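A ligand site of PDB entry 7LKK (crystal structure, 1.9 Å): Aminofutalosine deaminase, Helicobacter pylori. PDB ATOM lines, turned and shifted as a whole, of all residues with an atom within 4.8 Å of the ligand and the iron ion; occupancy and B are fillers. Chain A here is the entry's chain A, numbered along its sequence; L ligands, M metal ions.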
ATOM      1  N   HIS A  79       1.613  31.303 -34.936  1.00  0.00           N
ATOM      2  CA  HIS A  79       2.492  30.939 -33.823  1.00  0.00           C
ATOM      3  C   HIS A  79       2.754  32.171 -32.962  1.00  0.00           C
ATOM      4  O   HIS A  79       3.506  33.064 -33.372  1.00  0.00           O
ATOM      5  CB  HIS A  79       3.801  30.348 -34.338  1.00  0.00           C
ATOM      6  CG  HIS A  79       4.680  29.796 -33.265  1.00  0.00           C
ATOM      7  ND1 HIS A  79       4.515  28.529 -32.747  1.00  0.00           N
ATOM      8  CD2 HIS A  79       5.735  30.340 -32.601  1.00  0.00           C
ATOM      9  CE1 HIS A  79       5.431  28.313 -31.821  1.00  0.00           C
ATOM     10  NE2 HIS A  79       6.176  29.390 -31.713  1.00  0.00           N
ATOM     11  N   HIS A  81       2.972  33.377 -28.470  1.00  0.00           N
ATOM     12  CA  HIS A  81       2.955  33.011 -27.048  1.00  0.00           C
ATOM     13  C   HIS A  81       2.376  34.181 -26.260  1.00  0.00           C
ATOM     14  O   HIS A  81       3.108  35.070 -25.828  1.00  0.00           O
ATOM     15  CB  HIS A  81       4.366  32.657 -26.540  1.00  0.00           C
ATOM     16  CG  HIS A  81       5.032  31.562 -27.296  1.00  0.00           C
ATOM     17  ND1 HIS A  81       5.194  30.290 -26.791  1.00  0.00           N
ATOM     18  CD2 HIS A  81       5.603  31.542 -28.530  1.00  0.00           C
ATOM     19  CE1 HIS A  81       5.828  29.537 -27.669  1.00  0.00           C
ATOM     20  NE2 HIS A  81       6.085  30.268 -28.736  1.00  0.00           N
ATOM     21  N   PHE A  84       3.603  35.232 -22.533  1.00  0.00           N
ATOM     22  CA  PHE A  84       4.830  35.998 -22.335  1.00  0.00           C
ATOM     23  C   PHE A  84       4.682  37.454 -22.747  1.00  0.00           C
ATOM     24  O   PHE A  84       5.690  38.111 -23.037  1.00  0.00           O
ATOM     25  CB  PHE A  84       5.981  35.351 -23.107  1.00  0.00           C
ATOM     26  CG  PHE A  84       6.452  34.051 -22.521  1.00  0.00           C
ATOM     27  CD1 PHE A  84       7.395  34.023 -21.512  1.00  0.00           C
ATOM     28  CD2 PHE A  84       5.957  32.847 -23.006  1.00  0.00           C
ATOM     29  CE1 PHE A  84       7.841  32.826 -20.990  1.00  0.00           C
ATOM     30  CE2 PHE A  84       6.391  31.646 -22.474  1.00  0.00           C
ATOM     31  CZ  PHE A  84       7.332  31.635 -21.466  1.00  0.00           C
ATOM     32  N   PHE A  96      20.913  32.097 -28.773  1.00  0.00           N
ATOM     33  CA  PHE A  96      19.813  31.285 -28.280  1.00  0.00           C
ATOM     34  C   PHE A  96      20.092  30.785 -26.861  1.00  0.00           C
ATOM     35  O   PHE A  96      19.197  30.806 -26.013  1.00  0.00           O
ATOM     36  CB  PHE A  96      19.549  30.099 -29.207  1.00  0.00           C
ATOM     37  CG  PHE A  96      18.458  29.188 -28.727  1.00  0.00           C
ATOM     38  CD1 PHE A  96      17.137  29.464 -29.037  1.00  0.00           C
ATOM     39  CD2 PHE A  96      18.748  28.089 -27.939  1.00  0.00           C
ATOM     40  CE1 PHE A  96      16.124  28.634 -28.590  1.00  0.00           C
ATOM     41  CE2 PHE A  96      17.743  27.265 -27.490  1.00  0.00           C
ATOM     42  CZ  PHE A  96      16.428  27.541 -27.813  1.00  0.00           C
ATOM     43  N   TRP A  99      19.481  33.510 -24.504  1.00  0.00           N
ATOM     44  CA  TRP A  99      18.061  33.764 -24.346  1.00  0.00           C
ATOM     45  C   TRP A  99      17.399  32.694 -23.469  1.00  0.00           C
ATOM     46  O   TRP A  99      16.717  33.018 -22.497  1.00  0.00           O
ATOM     47  CB  TRP A  99      17.386  33.829 -25.721  1.00  0.00           C
ATOM     48  CG  TRP A  99      15.894  33.997 -25.650  1.00  0.00           C
ATOM     49  CD1 TRP A  99      15.209  35.166 -25.501  1.00  0.00           C
ATOM     50  CD2 TRP A  99      14.911  32.956 -25.716  1.00  0.00           C
ATOM     51  NE1 TRP A  99      13.857  34.925 -25.480  1.00  0.00           N
ATOM     52  CE2 TRP A  99      13.646  33.572 -25.601  1.00  0.00           C
ATOM     53  CE3 TRP A  99      14.969  31.567 -25.849  1.00  0.00           C
ATOM     54  CZ2 TRP A  99      12.457  32.850 -25.638  1.00  0.00           C
ATOM     55  CZ3 TRP A  99      13.788  30.851 -25.884  1.00  0.00           C
ATOM     56  CH2 TRP A  99      12.551  31.485 -25.774  1.00  0.00           C
ATOM     57  N   LEU A 100      17.623  31.422 -23.802  1.00  0.00           N
ATOM     58  CA  LEU A 100      16.967  30.341 -23.061  1.00  0.00           C
ATOM     59  C   LEU A 100      17.408  30.332 -21.598  1.00  0.00           C
ATOM     60  O   LEU A 100      16.574  30.151 -20.702  1.00  0.00           O
ATOM     61  CB  LEU A 100      17.266  28.996 -23.726  1.00  0.00           C
ATOM     62  CG  LEU A 100      16.584  27.764 -23.117  1.00  0.00           C
ATOM     63  CD1 LEU A 100      15.090  28.007 -22.921  1.00  0.00           C
ATOM     64  CD2 LEU A 100      16.821  26.540 -23.972  1.00  0.00           C
ATOM     65  N   VAL A 103      15.504  33.035 -19.858  1.00  0.00           N
ATOM     66  CA  VAL A 103      14.107  32.685 -19.648  1.00  0.00           C
ATOM     67  C   VAL A 103      13.966  31.775 -18.435  1.00  0.00           C
ATOM     68  O   VAL A 103      13.103  31.972 -17.570  1.00  0.00           O
ATOM     69  CB  VAL A 103      13.524  32.027 -20.911  1.00  0.00           C
ATOM     70  CG1 VAL A 103      12.134  31.464 -20.629  1.00  0.00           C
ATOM     71  CG2 VAL A 103      13.462  33.033 -22.063  1.00  0.00           C
ATOM     72  N   LEU A 104      14.840  30.761 -18.344  1.00  0.00           N
ATOM     73  CA  LEU A 104      14.774  29.834 -17.220  1.00  0.00           C
ATOM     74  C   LEU A 104      15.147  30.529 -15.920  1.00  0.00           C
ATOM     75  O   LEU A 104      14.487  30.325 -14.886  1.00  0.00           O
ATOM     76  CB  LEU A 104      15.688  28.641 -17.485  1.00  0.00           C
ATOM     77  CG  LEU A 104      15.235  27.714 -18.619  1.00  0.00           C
ATOM     78  CD1 LEU A 104      16.416  27.194 -19.401  1.00  0.00           C
ATOM     79  CD2 LEU A 104      14.407  26.564 -18.070  1.00  0.00           C
ATOM     80  N   ILE A 136       0.282  29.311 -28.684  1.00  0.00           N
ATOM     81  CA  ILE A 136       0.986  28.312 -27.872  1.00  0.00           C
ATOM     82  C   ILE A 136       0.783  28.650 -26.409  1.00  0.00           C
ATOM     83  O   ILE A 136       1.018  29.775 -25.969  1.00  0.00           O
ATOM     84  CB  ILE A 136       2.476  28.269 -28.231  1.00  0.00           C
ATOM     85  CG1 ILE A 136       2.665  28.009 -29.728  1.00  0.00           C
ATOM     86  CG2 ILE A 136       3.191  27.214 -27.395  1.00  0.00           C
ATOM     87  CD1 ILE A 136       2.648  26.538 -30.097  1.00  0.00           C
ATOM     88  N   ASN A 138       1.151  27.118 -22.257  1.00  0.00           N
ATOM     89  CA  ASN A 138       1.625  26.153 -21.277  1.00  0.00           C
ATOM     90  C   ASN A 138       0.684  25.999 -20.082  1.00  0.00           C
ATOM     91  O   ASN A 138       0.699  24.947 -19.440  1.00  0.00           O
ATOM     92  CB  ASN A 138       3.015  26.552 -20.768  1.00  0.00           C
ATOM     93  CG  ASN A 138       4.050  26.573 -21.866  1.00  0.00           C
ATOM     94  OD1 ASN A 138       4.706  27.594 -22.094  1.00  0.00           O
ATOM     95  ND2 ASN A 138       4.204  25.458 -22.564  1.00  0.00           N
ATOM     96  N   GLU A 158       1.016  23.236 -24.932  1.00  0.00           N
ATOM     97  CA  GLU A 158       2.390  22.830 -25.207  1.00  0.00           C
ATOM     98  C   GLU A 158       2.962  22.061 -24.021  1.00  0.00           C
ATOM     99  O   GLU A 158       2.915  22.551 -22.887  1.00  0.00           O
ATOM    100  CB  GLU A 158       3.260  24.050 -25.511  1.00  0.00           C
ATOM    101  CG  GLU A 158       4.732  23.734 -25.666  1.00  0.00           C
ATOM    102  CD  GLU A 158       5.556  24.973 -25.929  1.00  0.00           C
ATOM    103  OE1 GLU A 158       5.709  25.795 -25.002  1.00  0.00           O
ATOM    104  OE2 GLU A 158       6.040  25.126 -27.073  1.00  0.00           O
ATOM    105  N   LEU A 160       5.975  20.394 -21.829  1.00  0.00           N
ATOM    106  CA  LEU A 160       7.379  20.516 -21.450  1.00  0.00           C
ATOM    107  C   LEU A 160       7.720  19.394 -20.485  1.00  0.00           C
ATOM    108  O   LEU A 160       6.948  19.100 -19.570  1.00  0.00           O
ATOM    109  CB  LEU A 160       7.677  21.871 -20.790  1.00  0.00           C
ATOM    110  CG  LEU A 160       7.890  23.136 -21.619  1.00  0.00           C
ATOM    111  CD1 LEU A 160       9.238  23.088 -22.323  1.00  0.00           C
ATOM    112  CD2 LEU A 160       6.772  23.391 -22.611  1.00  0.00           C
ATOM    113  N   HIS A 194       7.254  20.809 -27.178  1.00  0.00           N
ATOM    114  CA  HIS A 194       8.040  22.035 -27.163  1.00  0.00           C
ATOM    115  C   HIS A 194       9.207  21.962 -28.137  1.00  0.00           C
ATOM    116  O   HIS A 194       9.297  22.742 -29.093  1.00  0.00           O
ATOM    117  CB  HIS A 194       8.536  22.354 -25.761  1.00  0.00           C
ATOM    118  CG  HIS A 194       9.405  23.581 -25.710  1.00  0.00           C
ATOM    119  ND1 HIS A 194      10.772  23.520 -25.619  1.00  0.00           N
ATOM    120  CD2 HIS A 194       9.087  24.889 -25.799  1.00  0.00           C
ATOM    121  CE1 HIS A 194      11.271  24.739 -25.628  1.00  0.00           C
ATOM    122  NE2 HIS A 194      10.264  25.595 -25.734  1.00  0.00           N
ATOM    123  N   TYR A 197      15.052  19.187 -27.358  1.00  0.00           N
ATOM    124  CA  TYR A 197      15.906  19.223 -26.182  1.00  0.00           C
ATOM    125  C   TYR A 197      15.129  19.275 -24.877  1.00  0.00           C
ATOM    126  O   TYR A 197      15.734  19.118 -23.804  1.00  0.00           O
ATOM    127  CB  TYR A 197      16.855  20.437 -26.244  1.00  0.00           C
ATOM    128  CG  TYR A 197      16.151  21.761 -26.445  1.00  0.00           C
ATOM    129  CD1 TYR A 197      15.505  22.406 -25.395  1.00  0.00           C
ATOM    130  CD2 TYR A 197      16.147  22.379 -27.693  1.00  0.00           C
ATOM    131  CE1 TYR A 197      14.871  23.612 -25.581  1.00  0.00           C
ATOM    132  CE2 TYR A 197      15.512  23.590 -27.888  1.00  0.00           C
ATOM    133  CZ  TYR A 197      14.875  24.202 -26.824  1.00  0.00           C
ATOM    134  OH  TYR A 197      14.233  25.407 -27.021  1.00  0.00           O
ATOM    135  N   SER A 198      13.821  19.488 -24.923  1.00  0.00           N
ATOM    136  CA  SER A 198      13.032  19.728 -23.729  1.00  0.00           C
ATOM    137  C   SER A 198      11.948  18.689 -23.453  1.00  0.00           C
ATOM    138  O   SER A 198      11.327  18.744 -22.389  1.00  0.00           O
ATOM    139  CB  SER A 198      12.365  21.111 -23.795  1.00  0.00           C
ATOM    140  OG  SER A 198      11.475  21.192 -24.886  1.00  0.00           O
ATOM    141  N   HIS A 221       8.714  23.291 -31.959  1.00  0.00           N
ATOM    142  CA  HIS A 221       9.903  24.054 -32.317  1.00  0.00           C
ATOM    143  C   HIS A 221      10.976  23.086 -32.799  1.00  0.00           C
ATOM    144  O   HIS A 221      11.243  22.081 -32.129  1.00  0.00           O
ATOM    145  CB  HIS A 221      10.414  24.877 -31.136  1.00  0.00           C
ATOM    146  CG  HIS A 221       9.400  25.825 -30.581  1.00  0.00           C
ATOM    147  ND1 HIS A 221       8.638  25.531 -29.469  1.00  0.00           N
ATOM    148  CD2 HIS A 221       9.033  27.065 -30.971  1.00  0.00           C
ATOM    149  CE1 HIS A 221       7.836  26.549 -29.206  1.00  0.00           C
ATOM    150  NE2 HIS A 221       8.065  27.490 -30.098  1.00  0.00           N
ATOM    151  N   GLU A 224      16.049  25.357 -34.035  1.00  0.00           N
ATOM    152  CA  GLU A 224      16.019  26.813 -33.948  1.00  0.00           C
ATOM    153  C   GLU A 224      17.400  27.410 -33.695  1.00  0.00           C
ATOM    154  O   GLU A 224      17.574  28.627 -33.859  1.00  0.00           O
ATOM    155  CB  GLU A 224      15.059  27.220 -32.831  1.00  0.00           C
ATOM    156  CG  GLU A 224      14.775  28.703 -32.716  1.00  0.00           C
ATOM    157  CD  GLU A 224      13.805  29.006 -31.589  1.00  0.00           C
ATOM    158  OE1 GLU A 224      13.406  28.066 -30.870  1.00  0.00           O
ATOM    159  OE2 GLU A 224      13.442  30.182 -31.433  1.00  0.00           O
ATOM    160  N   HIS A 275      10.407  27.601 -36.974  1.00  0.00           N
ATOM    161  CA  HIS A 275      11.787  28.088 -37.053  1.00  0.00           C
ATOM    162  C   HIS A 275      12.582  27.348 -38.133  1.00  0.00           C
ATOM    163  O   HIS A 275      12.608  27.795 -39.287  1.00  0.00           O
ATOM    164  CB  HIS A 275      12.474  27.999 -35.694  1.00  0.00           C
ATOM    165  CG  HIS A 275      11.757  28.760 -34.613  1.00  0.00           C
ATOM    166  ND1 HIS A 275      11.462  30.101 -34.732  1.00  0.00           N
ATOM    167  CD2 HIS A 275      11.257  28.367 -33.421  1.00  0.00           C
ATOM    168  CE1 HIS A 275      10.828  30.507 -33.637  1.00  0.00           C
ATOM    169  NE2 HIS A 275      10.691  29.468 -32.838  1.00  0.00           N
ATOM    170  N   SER A 302      12.199  36.958 -34.226  1.00  0.00           N
ATOM    171  CA  SER A 302      12.664  36.056 -33.184  1.00  0.00           C
ATOM    172  C   SER A 302      13.953  35.346 -33.590  1.00  0.00           C
ATOM    173  O   SER A 302      14.888  35.225 -32.786  1.00  0.00           O
ATOM    174  CB  SER A 302      11.580  35.035 -32.839  1.00  0.00           C
ATOM    175  OG  SER A 302      12.087  34.005 -32.018  1.00  0.00           O
ATOM    176  N   LEU A 306      17.518  35.633 -31.451  1.00  0.00           N
ATOM    177  CA  LEU A 306      18.029  34.468 -30.734  1.00  0.00           C
ATOM    178  C   LEU A 306      19.274  33.924 -31.410  1.00  0.00           C
ATOM    179  O   LEU A 306      20.383  34.402 -31.143  1.00  0.00           O
ATOM    180  CB  LEU A 306      16.939  33.384 -30.634  1.00  0.00           C
ATOM    181  CG  LEU A 306      16.057  33.405 -29.380  1.00  0.00           C
ATOM    182  CD1 LEU A 306      15.510  34.788 -29.102  1.00  0.00           C
ATOM    183  CD2 LEU A 306      14.924  32.388 -29.505  1.00  0.00           C
ATOM    184  N   ASP A 328       5.731  35.071 -33.354  1.00  0.00           N
ATOM    185  CA  ASP A 328       6.158  34.495 -32.082  1.00  0.00           C
ATOM    186  C   ASP A 328       5.571  35.345 -30.966  1.00  0.00           C
ATOM    187  O   ASP A 328       4.592  36.067 -31.167  1.00  0.00           O
ATOM    188  CB  ASP A 328       7.683  34.424 -31.984  1.00  0.00           C
ATOM    189  CG  ASP A 328       8.171  33.091 -31.442  1.00  0.00           C
ATOM    190  OD1 ASP A 328       7.349  32.349 -30.865  1.00  0.00           O
ATOM    191  OD2 ASP A 328       9.375  32.790 -31.574  1.00  0.00           O
ATOM    192  N   SER A 331       8.195  37.462 -25.863  1.00  0.00           N
ATOM    193  CA  SER A 331       9.393  36.879 -25.284  1.00  0.00           C
ATOM    194  C   SER A 331      10.565  36.881 -26.261  1.00  0.00           C
ATOM    195  O   SER A 331      11.718  36.731 -25.831  1.00  0.00           O
ATOM    196  CB  SER A 331       9.112  35.440 -24.828  1.00  0.00           C
ATOM    197  OG  SER A 331       8.216  34.795 -25.724  1.00  0.00           O
ATOM    198  N   SER A 332      10.296  37.050 -27.561  1.00  0.00           N
ATOM    199  CA  SER A 332      11.357  37.063 -28.563  1.00  0.00           C
ATOM    200  C   SER A 332      10.991  37.993 -29.718  1.00  0.00           C
ATOM    201  O   SER A 332      11.243  37.694 -30.885  1.00  0.00           O
ATOM    202  CB  SER A 332      11.646  35.654 -29.089  1.00  0.00           C
ATOM    203  OG  SER A 332      10.443  35.001 -29.470  1.00  0.00           O
HETATM  204  O1  LIG L   1       9.389  29.843 -29.906  1.00  0.00           O
HETATM  205  C1  LIG L   1      10.002  30.854 -29.142  1.00  0.00           C
HETATM  206  C2  LIG L   1      11.505  30.651 -29.013  1.00  0.00           C
HETATM  207  N1  LIG L   1      11.850  29.248 -29.030  1.00  0.00           N
HETATM  208  C3  LIG L   1      11.149  28.346 -28.143  1.00  0.00           C
HETATM  209  N2  LIG L   1      10.083  28.703 -27.215  1.00  0.00           N
HETATM  210  C4  LIG L   1       9.421  29.973 -26.847  1.00  0.00           C
HETATM  211  C5  LIG L   1       9.346  31.017 -27.754  1.00  0.00           C
HETATM  212  N3  LIG L   1       8.705  32.012 -27.165  1.00  0.00           N
HETATM  213  C6  LIG L   1       8.344  31.650 -25.938  1.00  0.00           C
HETATM  214  N4  LIG L   1       8.780  30.402 -25.749  1.00  0.00           N
HETATM  215  C7  LIG L   1       8.571  29.651 -24.468  1.00  0.00           C
HETATM  216  C8  LIG L   1       8.148  28.180 -24.664  1.00  0.00           C
HETATM  217  O2  LIG L   1       6.796  28.089 -24.847  1.00  0.00           O
HETATM  218  O3  LIG L   1       9.684  29.569 -23.829  1.00  0.00           O
HETATM  219  C9  LIG L   1       9.563  28.240 -22.910  1.00  0.00           C
HETATM  220  C10 LIG L   1       8.554  27.543 -23.342  1.00  0.00           C
HETATM  221  O4  LIG L   1       7.423  27.648 -22.355  1.00  0.00           O
HETATM  222  C11 LIG L   1      10.846  27.445 -23.027  1.00  0.00           C
HETATM  223  S1  LIG L   1      11.153  26.540 -21.475  1.00  0.00           S
HETATM  224  C12 LIG L   1      12.314  25.178 -21.791  1.00  0.00           C
HETATM  225 FE    FE M   1       7.434  29.778 -30.119  1.00  0.00          FE
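The iron ion is bound by O1 of the ligand (2.0 Å), NE2 of His 81 (2.0 Å), NE2 of His 79 (2.1 Å) and NE2 of His 221 (2.4 Å). Slightly farther from the iron ion lies OD1 of Asp 328 (2.7 Å).
Of the 23 residues printed, 4 come within 4 Å of the iron ion.
Merely in contact with the ligand: Phe 84 (3.6 Å), Trp 99 (3.5 Å), Leu 160 (3.8 Å) and Leu 306 (3.9 Å). 14 residues have an atom within 4 Å of the ligand: His 79, His 81, Phe 84, Trp 99, Asn 138, Glu 158, Leu 160, His 194, His 221, Glu 224, His 275, Leu 306, Asp 328 and Ser 331. The nearest printed residue that does not touch the ligand is Leu 100 (4.1 Å).
An oxygen (O2) of the ligand lies within hydrogen-bond range of the side-chain carboxylate (OE1) of Glu 158, 2.5 Å away. A ring nitrogen (NE2) of His 194 sits close to a nitrogen (N2) of the ligand (3.4 Å). The side-chain amide oxygen (OD1) of Asn 138 sits at hydrogen-bond distance from an oxygen (O4) of the ligand (2.7 Å). The side-chain carboxylate (OE1) of Glu 224 sits at hydrogen-bond distance from a nitrogen (N1) of the ligand (2.7 Å). The side-chain carboxylate of Asp 328 sits close to an oxygen (O1) of the ligand (3.4 Å). NE2 of His 275 sits close to O1 of the ligand, 3.2 Å away. OG of Ser 331 sits close to N3 of the ligand (3.2 Å).
The side-chain carboxylate of Asp 328 sits at hydrogen-bond distance from the side-chain hydroxyl of Ser 302, at 3.0 Å. OG of Ser 198 lies within hydrogen-bond range of ND1 of His 194 (2.5 Å). The backbone NH (N) of Phe 96 is in hydrogen-bond range of the backbone carbonyl oxygen (O) of Leu 306 (3.3 Å). A ring nitrogen (NE2) of His 81 lies close to the side-chain carboxylate of Asp 328. The backbone carbonyl oxygen of His 194 lies within hydrogen-bond range of a ring nitrogen (ND1) of His 221 (2.9 Å). OE2 of Glu 224 lies within hydrogen-bond range of NE2 of His 275. NE1 of Trp 99 sits at hydrogen-bond distance from O of Ser 331 (2.8 Å). The side-chain carboxylate of Glu 158 sits at hydrogen-bond distance from the side-chain amide nitrogen of Asn 138.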
